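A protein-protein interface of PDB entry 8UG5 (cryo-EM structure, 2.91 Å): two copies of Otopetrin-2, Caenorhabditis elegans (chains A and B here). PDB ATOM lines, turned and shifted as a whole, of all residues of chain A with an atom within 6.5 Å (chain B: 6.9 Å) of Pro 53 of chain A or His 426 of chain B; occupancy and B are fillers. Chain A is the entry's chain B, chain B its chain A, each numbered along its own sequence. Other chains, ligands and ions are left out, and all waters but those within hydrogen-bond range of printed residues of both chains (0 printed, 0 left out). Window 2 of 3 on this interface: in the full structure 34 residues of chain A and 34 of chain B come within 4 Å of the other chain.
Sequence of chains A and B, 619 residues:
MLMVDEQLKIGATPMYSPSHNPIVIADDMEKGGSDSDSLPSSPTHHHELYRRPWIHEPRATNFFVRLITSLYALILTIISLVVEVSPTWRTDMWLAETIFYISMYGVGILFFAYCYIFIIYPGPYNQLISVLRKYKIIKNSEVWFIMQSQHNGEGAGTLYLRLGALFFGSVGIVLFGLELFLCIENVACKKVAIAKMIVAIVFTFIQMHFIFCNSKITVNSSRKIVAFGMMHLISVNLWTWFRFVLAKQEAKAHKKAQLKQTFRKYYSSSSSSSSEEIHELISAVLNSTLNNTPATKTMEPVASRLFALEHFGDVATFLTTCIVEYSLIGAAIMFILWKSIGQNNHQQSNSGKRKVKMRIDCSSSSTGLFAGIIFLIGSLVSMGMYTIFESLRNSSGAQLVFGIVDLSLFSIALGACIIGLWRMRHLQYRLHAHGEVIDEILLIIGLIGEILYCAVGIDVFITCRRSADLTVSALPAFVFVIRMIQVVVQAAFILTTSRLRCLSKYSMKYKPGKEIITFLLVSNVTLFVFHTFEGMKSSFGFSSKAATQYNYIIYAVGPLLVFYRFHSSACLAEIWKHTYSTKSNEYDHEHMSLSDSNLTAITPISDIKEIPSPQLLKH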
ATOM      1  N   ARG A  51      16.249  -8.935  -6.725  1.00  0.00           N
ATOM      2  CA  ARG A  51      17.038  -9.305  -5.560  1.00  0.00           C
ATOM      3  C   ARG A  51      17.448  -8.096  -4.736  1.00  0.00           C
ATOM      4  O   ARG A  51      18.013  -8.270  -3.652  1.00  0.00           O
ATOM      5  CB  ARG A  51      18.296 -10.093  -5.960  1.00  0.00           C
ATOM      6  CG  ARG A  51      19.330  -9.291  -6.730  1.00  0.00           C
ATOM      7  CD  ARG A  51      20.490 -10.163  -7.170  1.00  0.00           C
ATOM      8  NE  ARG A  51      20.114 -11.139  -8.181  1.00  0.00           N
ATOM      9  CZ  ARG A  51      20.912 -12.104  -8.616  1.00  0.00           C
ATOM     10  NH1 ARG A  51      22.146 -12.239  -8.158  1.00  0.00           N
ATOM     11  NH2 ARG A  51      20.462 -12.953  -9.537  1.00  0.00           N
ATOM     12  N   ARG A  52      17.179  -6.885  -5.214  1.00  0.00           N
ATOM     13  CA  ARG A  52      17.597  -5.685  -4.512  1.00  0.00           C
ATOM     14  C   ARG A  52      16.796  -5.504  -3.223  1.00  0.00           C
ATOM     15  O   ARG A  52      15.674  -6.003  -3.102  1.00  0.00           O
ATOM     16  CB  ARG A  52      17.422  -4.458  -5.398  1.00  0.00           C
ATOM     17  CG  ARG A  52      15.976  -4.162  -5.743  1.00  0.00           C
ATOM     18  CD  ARG A  52      15.857  -2.918  -6.593  1.00  0.00           C
ATOM     19  NE  ARG A  52      16.510  -3.089  -7.884  1.00  0.00           N
ATOM     20  CZ  ARG A  52      15.928  -3.596  -8.962  1.00  0.00           C
ATOM     21  NH1 ARG A  52      14.688  -4.049  -8.929  1.00  0.00           N
ATOM     22  NH2 ARG A  52      16.615  -3.656 -10.099  1.00  0.00           N
ATOM     23  N   PRO A  53      17.358  -4.803  -2.244  1.00  0.00           N
ATOM     24  CA  PRO A  53      16.596  -4.486  -1.033  1.00  0.00           C
ATOM     25  C   PRO A  53      15.432  -3.557  -1.334  1.00  0.00           C
ATOM     26  O   PRO A  53      15.456  -2.781  -2.293  1.00  0.00           O
ATOM     27  CB  PRO A  53      17.628  -3.804  -0.127  1.00  0.00           C
ATOM     28  CG  PRO A  53      18.957  -4.182  -0.692  1.00  0.00           C
ATOM     29  CD  PRO A  53      18.751  -4.340  -2.157  1.00  0.00           C
ATOM     30  N   TRP A  54      14.398  -3.646  -0.495  1.00  0.00           N
ATOM     31  CA  TRP A  54      13.231  -2.789  -0.672  1.00  0.00           C
ATOM     32  C   TRP A  54      13.548  -1.320  -0.445  1.00  0.00           C
ATOM     33  O   TRP A  54      12.810  -0.456  -0.932  1.00  0.00           O
ATOM     34  CB  TRP A  54      12.106  -3.220   0.268  1.00  0.00           C
ATOM     35  CG  TRP A  54      12.322  -2.859   1.706  1.00  0.00           C
ATOM     36  CD1 TRP A  54      12.987  -3.593   2.638  1.00  0.00           C
ATOM     37  CD2 TRP A  54      11.849  -1.688   2.383  1.00  0.00           C
ATOM     38  NE1 TRP A  54      12.967  -2.954   3.850  1.00  0.00           N
ATOM     39  CE2 TRP A  54      12.274  -1.780   3.721  1.00  0.00           C
ATOM     40  CE3 TRP A  54      11.110  -0.571   1.986  1.00  0.00           C
ATOM     41  CZ2 TRP A  54      11.988  -0.799   4.664  1.00  0.00           C
ATOM     42  CZ3 TRP A  54      10.829   0.404   2.925  1.00  0.00           C
ATOM     43  CH2 TRP A  54      11.267   0.283   4.248  1.00  0.00           C
ATOM     44  N   ILE A  55      14.619  -1.010   0.287  1.00  0.00           N
ATOM     45  CA  ILE A  55      15.006   0.384   0.456  1.00  0.00           C
ATOM     46  C   ILE A  55      15.512   0.962  -0.859  1.00  0.00           C
ATOM     47  O   ILE A  55      15.600   2.184  -1.013  1.00  0.00           O
ATOM     48  CB  ILE A  55      16.048   0.516   1.580  1.00  0.00           C
ATOM     49  CG1 ILE A  55      17.318  -0.258   1.229  1.00  0.00           C
ATOM     50  CG2 ILE A  55      15.470   0.027   2.895  1.00  0.00           C
ATOM     51  CD1 ILE A  55      18.462   0.014   2.175  1.00  0.00           C
ATOM     52  N   HIS A  56      15.642   0.147  -1.876  1.00  0.00           N
ATOM     53  CA  HIS A  56      16.199   0.613  -3.155  1.00  0.00           C
ATOM     54  C   HIS A  56      15.271   0.162  -4.280  1.00  0.00           C
ATOM     55  O   HIS A  56      15.631   0.320  -5.447  1.00  0.00           O
ATOM     56  CB  HIS A  56      17.634   0.104  -3.332  1.00  0.00           C
ATOM     57  CG  HIS A  56      18.651   0.700  -2.430  1.00  0.00           C
ATOM     58  ND1 HIS A  56      19.518  -0.081  -1.699  1.00  0.00           N
ATOM     59  CD2 HIS A  56      18.954   1.963  -2.140  1.00  0.00           C
ATOM     60  CE1 HIS A  56      20.312   0.700  -0.989  1.00  0.00           C
ATOM     61  NE2 HIS A  56      19.988   1.947  -1.242  1.00  0.00           N
ATOM     62  N   GLU A  57      14.077  -0.316  -3.910  1.00  0.00           N
ATOM     63  CA  GLU A  57      13.045  -0.678  -4.913  1.00  0.00           C
ATOM     64  C   GLU A  57      12.074   0.502  -5.026  1.00  0.00           C
ATOM     65  O   GLU A  57      11.447   0.834  -4.005  1.00  0.00           O
ATOM     66  CB  GLU A  57      12.228  -1.874  -4.434  1.00  0.00           C
ATOM     67  CG  GLU A  57      12.846  -3.221  -4.728  1.00  0.00           C
ATOM     68  CD  GLU A  57      12.279  -3.911  -5.956  1.00  0.00           C
ATOM     69  OE1 GLU A  57      12.607  -5.093  -6.171  1.00  0.00           O
ATOM     70  OE2 GLU A  57      11.510  -3.263  -6.693  1.00  0.00           O
ATOM     71  N   ALA A  60       8.619   0.141  -3.640  1.00  0.00           N
ATOM     72  CA  ALA A  60       8.692  -0.228  -2.220  1.00  0.00           C
ATOM     73  C   ALA A  60       8.921   1.061  -1.465  1.00  0.00           C
ATOM     74  O   ALA A  60       8.282   1.258  -0.421  1.00  0.00           O
ATOM     75  CB  ALA A  60       9.811  -1.184  -2.028  1.00  0.00           C
ATOM     76  N   LEU B 421      12.976  -3.059  11.658  1.00  0.00           N
ATOM     77  CA  LEU B 421      13.006  -2.371  10.372  1.00  0.00           C
ATOM     78  C   LEU B 421      14.434  -2.216   9.869  1.00  0.00           C
ATOM     79  O   LEU B 421      14.696  -2.353   8.669  1.00  0.00           O
ATOM     80  CB  LEU B 421      12.324  -1.009  10.491  1.00  0.00           C
ATOM     81  CG  LEU B 421      10.833  -0.968  10.159  1.00  0.00           C
ATOM     82  CD1 LEU B 421      10.196   0.301  10.693  1.00  0.00           C
ATOM     83  CD2 LEU B 421      10.628  -1.078   8.657  1.00  0.00           C
ATOM     84  N   TRP B 422      15.373  -1.924  10.773  1.00  0.00           N
ATOM     85  CA  TRP B 422      16.773  -1.839  10.378  1.00  0.00           C
ATOM     86  C   TRP B 422      17.310  -3.193   9.929  1.00  0.00           C
ATOM     87  O   TRP B 422      18.054  -3.278   8.947  1.00  0.00           O
ATOM     88  CB  TRP B 422      17.614  -1.292  11.528  1.00  0.00           C
ATOM     89  CG  TRP B 422      19.031  -1.010  11.140  1.00  0.00           C
ATOM     90  CD1 TRP B 422      20.151  -1.538  11.703  1.00  0.00           C
ATOM     91  CD2 TRP B 422      19.479  -0.114  10.116  1.00  0.00           C
ATOM     92  NE1 TRP B 422      21.272  -1.040  11.084  1.00  0.00           N
ATOM     93  CE2 TRP B 422      20.886  -0.161  10.107  1.00  0.00           C
ATOM     94  CE3 TRP B 422      18.827   0.720   9.201  1.00  0.00           C
ATOM     95  CZ2 TRP B 422      21.651   0.593   9.223  1.00  0.00           C
ATOM     96  CZ3 TRP B 422      19.589   1.467   8.323  1.00  0.00           C
ATOM     97  CH2 TRP B 422      20.985   1.399   8.340  1.00  0.00           C
ATOM     98  N   ARG B 423      16.955  -4.263  10.643  1.00  0.00           N
ATOM     99  CA  ARG B 423      17.469  -5.583  10.288  1.00  0.00           C
ATOM    100  C   ARG B 423      16.840  -6.101   9.002  1.00  0.00           C
ATOM    101  O   ARG B 423      17.517  -6.743   8.192  1.00  0.00           O
ATOM    102  CB  ARG B 423      17.230  -6.574  11.428  1.00  0.00           C
ATOM    103  CG  ARG B 423      17.693  -6.089  12.788  1.00  0.00           C
ATOM    104  CD  ARG B 423      19.095  -6.564  13.120  1.00  0.00           C
ATOM    105  NE  ARG B 423      19.139  -7.990  13.420  1.00  0.00           N
ATOM    106  CZ  ARG B 423      20.118  -8.802  13.046  1.00  0.00           C
ATOM    107  NH1 ARG B 423      21.151  -8.361  12.348  1.00  0.00           N
ATOM    108  NH2 ARG B 423      20.058 -10.088  13.382  1.00  0.00           N
ATOM    109  N   MET B 424      15.555  -5.822   8.796  1.00  0.00           N
ATOM    110  CA  MET B 424      14.802  -6.347   7.667  1.00  0.00           C
ATOM    111  C   MET B 424      14.877  -5.446   6.441  1.00  0.00           C
ATOM    112  O   MET B 424      14.125  -5.657   5.482  1.00  0.00           O
ATOM    113  CB  MET B 424      13.346  -6.563   8.079  1.00  0.00           C
ATOM    114  CG  MET B 424      13.170  -7.657   9.120  1.00  0.00           C
ATOM    115  SD  MET B 424      11.469  -7.856   9.676  1.00  0.00           S
ATOM    116  CE  MET B 424      10.714  -8.565   8.223  1.00  0.00           C
ATOM    117  N   ARG B 425      15.769  -4.456   6.446  1.00  0.00           N
ATOM    118  CA  ARG B 425      15.887  -3.533   5.325  1.00  0.00           C
ATOM    119  C   ARG B 425      16.401  -4.203   4.059  1.00  0.00           C
ATOM    120  O   ARG B 425      16.257  -3.632   2.974  1.00  0.00           O
ATOM    121  CB  ARG B 425      16.815  -2.373   5.689  1.00  0.00           C
ATOM    122  CG  ARG B 425      18.273  -2.777   5.834  1.00  0.00           C
ATOM    123  CD  ARG B 425      19.134  -1.625   6.330  1.00  0.00           C
ATOM    124  NE  ARG B 425      20.547  -1.980   6.371  1.00  0.00           N
ATOM    125  CZ  ARG B 425      21.140  -2.578   7.395  1.00  0.00           C
ATOM    126  NH1 ARG B 425      20.470  -2.912   8.485  1.00  0.00           N
ATOM    127  NH2 ARG B 425      22.440  -2.853   7.322  1.00  0.00           N
ATOM    128  N   HIS B 426      16.991  -5.390   4.167  1.00  0.00           N
ATOM    129  CA  HIS B 426      17.608  -6.059   3.031  1.00  0.00           C
ATOM    130  C   HIS B 426      16.678  -7.041   2.331  1.00  0.00           C
ATOM    131  O   HIS B 426      17.100  -7.695   1.373  1.00  0.00           O
ATOM    132  CB  HIS B 426      18.881  -6.779   3.476  1.00  0.00           C
ATOM    133  CG  HIS B 426      20.038  -5.862   3.716  1.00  0.00           C
ATOM    134  ND1 HIS B 426      20.280  -4.750   2.939  1.00  0.00           N
ATOM    135  CD2 HIS B 426      21.024  -5.892   4.644  1.00  0.00           C
ATOM    136  CE1 HIS B 426      21.362  -4.134   3.379  1.00  0.00           C
ATOM    137  NE2 HIS B 426      21.833  -4.807   4.413  1.00  0.00           N
ATOM    138  N   LEU B 427      15.432  -7.161   2.778  1.00  0.00           N
ATOM    139  CA  LEU B 427      14.482  -8.047   2.126  1.00  0.00           C
ATOM    140  C   LEU B 427      13.974  -7.415   0.833  1.00  0.00           C
ATOM    141  O   LEU B 427      14.433  -6.356   0.404  1.00  0.00           O
ATOM    142  CB  LEU B 427      13.331  -8.380   3.071  1.00  0.00           C
ATOM    143  CG  LEU B 427      13.750  -8.883   4.450  1.00  0.00           C
ATOM    144  CD1 LEU B 427      12.529  -9.216   5.270  1.00  0.00           C
ATOM    145  CD2 LEU B 427      14.646 -10.100   4.313  1.00  0.00           C
ATOM    146  N   GLN B 428      13.008  -8.073   0.201  1.00  0.00           N
ATOM    147  CA  GLN B 428      12.508  -7.652  -1.096  1.00  0.00           C
ATOM    148  C   GLN B 428      11.015  -7.366  -1.019  1.00  0.00           C
ATOM    149  O   GLN B 428      10.282  -7.999  -0.255  1.00  0.00           O
ATOM    150  CB  GLN B 428      12.777  -8.714  -2.174  1.00  0.00           C
ATOM    151  CG  GLN B 428      14.254  -9.018  -2.425  1.00  0.00           C
ATOM    152  CD  GLN B 428      14.906  -9.773  -1.286  1.00  0.00           C
ATOM    153  OE1 GLN B 428      14.227 -10.282  -0.396  1.00  0.00           O
ATOM    154  NE2 GLN B 428      16.230  -9.840  -1.301  1.00  0.00           N
ATOM    155  N   TYR B 429      10.591  -6.405  -1.846  1.00  0.00           N
ATOM    156  CA  TYR B 429       9.152  -6.066  -1.927  1.00  0.00           C
ATOM    157  C   TYR B 429       8.412  -7.244  -2.554  1.00  0.00           C
ATOM    158  O   TYR B 429       8.965  -7.897  -3.459  1.00  0.00           O
ATOM    159  CB  TYR B 429       8.956  -4.822  -2.794  1.00  0.00           C
ATOM    160  CG  TYR B 429       7.701  -4.038  -2.515  1.00  0.00           C
ATOM    161  CD1 TYR B 429       7.187  -3.946  -1.233  1.00  0.00           C
ATOM    162  CD2 TYR B 429       7.036  -3.372  -3.531  1.00  0.00           C
ATOM    163  CE1 TYR B 429       6.042  -3.215  -0.968  1.00  0.00           C
ATOM    164  CE2 TYR B 429       5.890  -2.636  -3.283  1.00  0.00           C
ATOM    165  CZ  TYR B 429       5.392  -2.557  -1.996  1.00  0.00           C
ATOM    166  OH  TYR B 429       4.251  -1.837  -1.740  1.00  0.00           O
ATOM    167  N   LEU B 500       7.089  -7.581   2.806  1.00  0.00           N
ATOM    168  CA  LEU B 500       8.489  -7.948   2.649  1.00  0.00           C
ATOM    169  C   LEU B 500       8.636  -9.460   2.726  1.00  0.00           C
ATOM    170  O   LEU B 500       8.109 -10.093   3.646  1.00  0.00           O
ATOM    171  CB  LEU B 500       9.344  -7.278   3.721  1.00  0.00           C
ATOM    172  CG  LEU B 500       9.614  -5.800   3.469  1.00  0.00           C
ATOM    173  CD1 LEU B 500      10.585  -5.257   4.500  1.00  0.00           C
ATOM    174  CD2 LEU B 500      10.145  -5.611   2.067  1.00  0.00           C
ATOM    175  N   ARG B 501       9.349 -10.032   1.764  1.00  0.00           N
ATOM    176  CA  ARG B 501       9.559 -11.467   1.698  1.00  0.00           C
ATOM    177  C   ARG B 501      11.037 -11.763   1.501  1.00  0.00           C
ATOM    178  O   ARG B 501      11.760 -11.000   0.857  1.00  0.00           O
ATOM    179  CB  ARG B 501       8.749 -12.103   0.564  1.00  0.00           C
ATOM    180  CG  ARG B 501       7.305 -12.391   0.929  1.00  0.00           C
ATOM    181  CD  ARG B 501       6.441 -11.177   0.674  1.00  0.00           C
ATOM    182  NE  ARG B 501       5.038 -11.521   0.489  1.00  0.00           N
ATOM    183  CZ  ARG B 501       4.105 -11.374   1.419  1.00  0.00           C
ATOM    184  NH1 ARG B 501       4.367 -10.775   2.569  1.00  0.00           N
ATOM    185  NH2 ARG B 501       2.882 -11.836   1.188  1.00  0.00           N
ATOM    186  N   SER B 504      15.959 -13.439  -1.327  1.00  0.00           N
ATOM    187  CA  SER B 504      17.407 -13.508  -1.660  1.00  0.00           C
ATOM    188  C   SER B 504      18.014 -14.786  -1.076  1.00  0.00           C
ATOM    189  O   SER B 504      17.511 -15.254  -0.044  1.00  0.00           O
ATOM    190  CB  SER B 504      18.151 -12.300  -1.168  1.00  0.00           C
ATOM    191  OG  SER B 504      19.505 -12.335  -1.597  1.00  0.00           O
ATOM    192  N   TYR B 506      20.716 -15.169   0.633  1.00  0.00           N
ATOM    193  CA  TYR B 506      21.015 -14.833   2.048  1.00  0.00           C
ATOM    194  C   TYR B 506      19.697 -14.654   2.807  1.00  0.00           C
ATOM    195  O   TYR B 506      19.564 -15.214   3.906  1.00  0.00           O
ATOM    196  CB  TYR B 506      21.915 -13.594   2.121  1.00  0.00           C
ATOM    197  CG  TYR B 506      22.223 -13.083   3.507  1.00  0.00           C
ATOM    198  CD1 TYR B 506      23.153 -13.716   4.315  1.00  0.00           C
ATOM    199  CD2 TYR B 506      21.597 -11.953   4.008  1.00  0.00           C
ATOM    200  CE1 TYR B 506      23.442 -13.252   5.587  1.00  0.00           C
ATOM    201  CE2 TYR B 506      21.872 -11.476   5.278  1.00  0.00           C
ATOM    202  CZ  TYR B 506      22.801 -12.126   6.070  1.00  0.00           C
ATOM    203  OH  TYR B 506      23.088 -11.660   7.329  1.00  0.00           O
ATOM    204  N   SER B 507      18.749 -13.910   2.232  1.00  0.00           N
ATOM    205  CA  SER B 507      17.487 -13.618   2.959  1.00  0.00           C
ATOM    206  C   SER B 507      16.779 -14.934   3.291  1.00  0.00           C
ATOM    207  O   SER B 507      16.223 -15.044   4.394  1.00  0.00           O
ATOM    208  CB  SER B 507      16.602 -12.700   2.161  1.00  0.00           C
ATOM    209  OG  SER B 507      17.141 -11.388   2.122  1.00  0.00           O
ATOM    210  N   PRO B 512      16.430 -12.809   7.935  1.00  0.00           N
ATOM    211  CA  PRO B 512      16.713 -11.628   8.759  1.00  0.00           C
ATOM    212  C   PRO B 512      15.475 -11.065   9.465  1.00  0.00           C
ATOM    213  O   PRO B 512      14.523 -10.740   8.781  1.00  0.00           O
ATOM    214  CB  PRO B 512      17.208 -10.576   7.754  1.00  0.00           C
ATOM    215  CG  PRO B 512      17.575 -11.362   6.515  1.00  0.00           C
ATOM    216  CD  PRO B 512      16.639 -12.547   6.511  1.00  0.00           C
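O of Met 424 of chain B lies within hydrogen-bond range of NE1 of Trp 54 of chain A, 3.4 Å away. The indole nitrogen (NE1) of Trp 54 of chain A sits close to the backbone carbonyl oxygen (O) of Arg 425 of chain B (3.5 Å). The backbone carbonyl oxygen (O) of Leu 427 of chain B is in hydrogen-bond range of the backbone NH (N) of Trp 54 of chain A (2.9 Å). The backbone carbonyl oxygen (O) of Arg 51 of chain A lies within hydrogen-bond range of the side-chain amide nitrogen (NE2) of Gln 428 of chain B (3.3 Å).
Pro 53 of chain A touches just these residues of chain B: Arg 425 (3.4 Å), His 426 (3.9 Å) and Leu 427 (3.2 Å). Of chain A, only Pro 53 (3.9 Å) comes within 4 Å of His 426 of chain B. Of the printed residues of chain A, Met 424 of chain B touches Trp 54. Printed residues of chain B within 4 Å of Arg 51 of chain A: Gln 428 (3.3 Å). Of the printed residues of chain A, Gln 428 of chain B touches Arg 51 (3.3 Å) and Arg 52 (3.4 Å). Printed residues of chain B within 4 Å of Arg 52 of chain A: Leu 427 (3.7 Å) and Gln 428 (3.4 Å). Glu 57 of chain A touches none of the printed residues of chain B. The nearest residue of chain A that does not touch His 426 of chain B is Trp 54 of chain A (4.6 Å). The nearest printed residue of chain A that does not touch Tyr 429 of chain B is Trp 54 of chain A (4.1 Å).
Leu 427 of chain B touches Arg 52 of chain A (O to O, 3.7 Å). Arg 52 of chain A touches Gln 428 of chain B (O to CG, 3.4 Å). O of Arg 425 of chain B touches CB of Pro 53 of chain A (3.4 Å). Pro 53 of chain A touches His 426 of chain B (CB to CA, 3.9 Å). Leu 427 of chain B touches Pro 53 of chain A. Trp 54 of chain A touches Leu 500 of chain B. Arg 425 of chain B touches Ile 55 of chain A (O to CG2, 3.7 Å). CG of Tyr 429 of chain B touches CB of Ala 60 of chain A (3.6 Å).
Of the 15 printed residues of chain B, 7 touch a printed residue of chain A. Among the printed residues, 12 pairs touch across the chains. Among the printed residues, no Asp or Glu carboxylate lies within 4 Å of a Lys or Arg side-chain nitrogen of the other chain.
No position is printed for both chains. Of the 12 pairs that touch across the chains among the printed residues, none has its exchanged pair printed and touching as well.
The backbone carbonyl oxygen of Trp 422 of chain B lies within hydrogen-bond range of the guanidinium group of Arg 425 of chain B, 2.5 Å away. O of Arg 501 of chain B sits close to OE1 of Gln 428 of chain B, 2.9 Å away. The side-chain carboxylate of Glu 57 of chain A is in salt-bridge range of the guanidinium group of Arg 52 of chain A.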
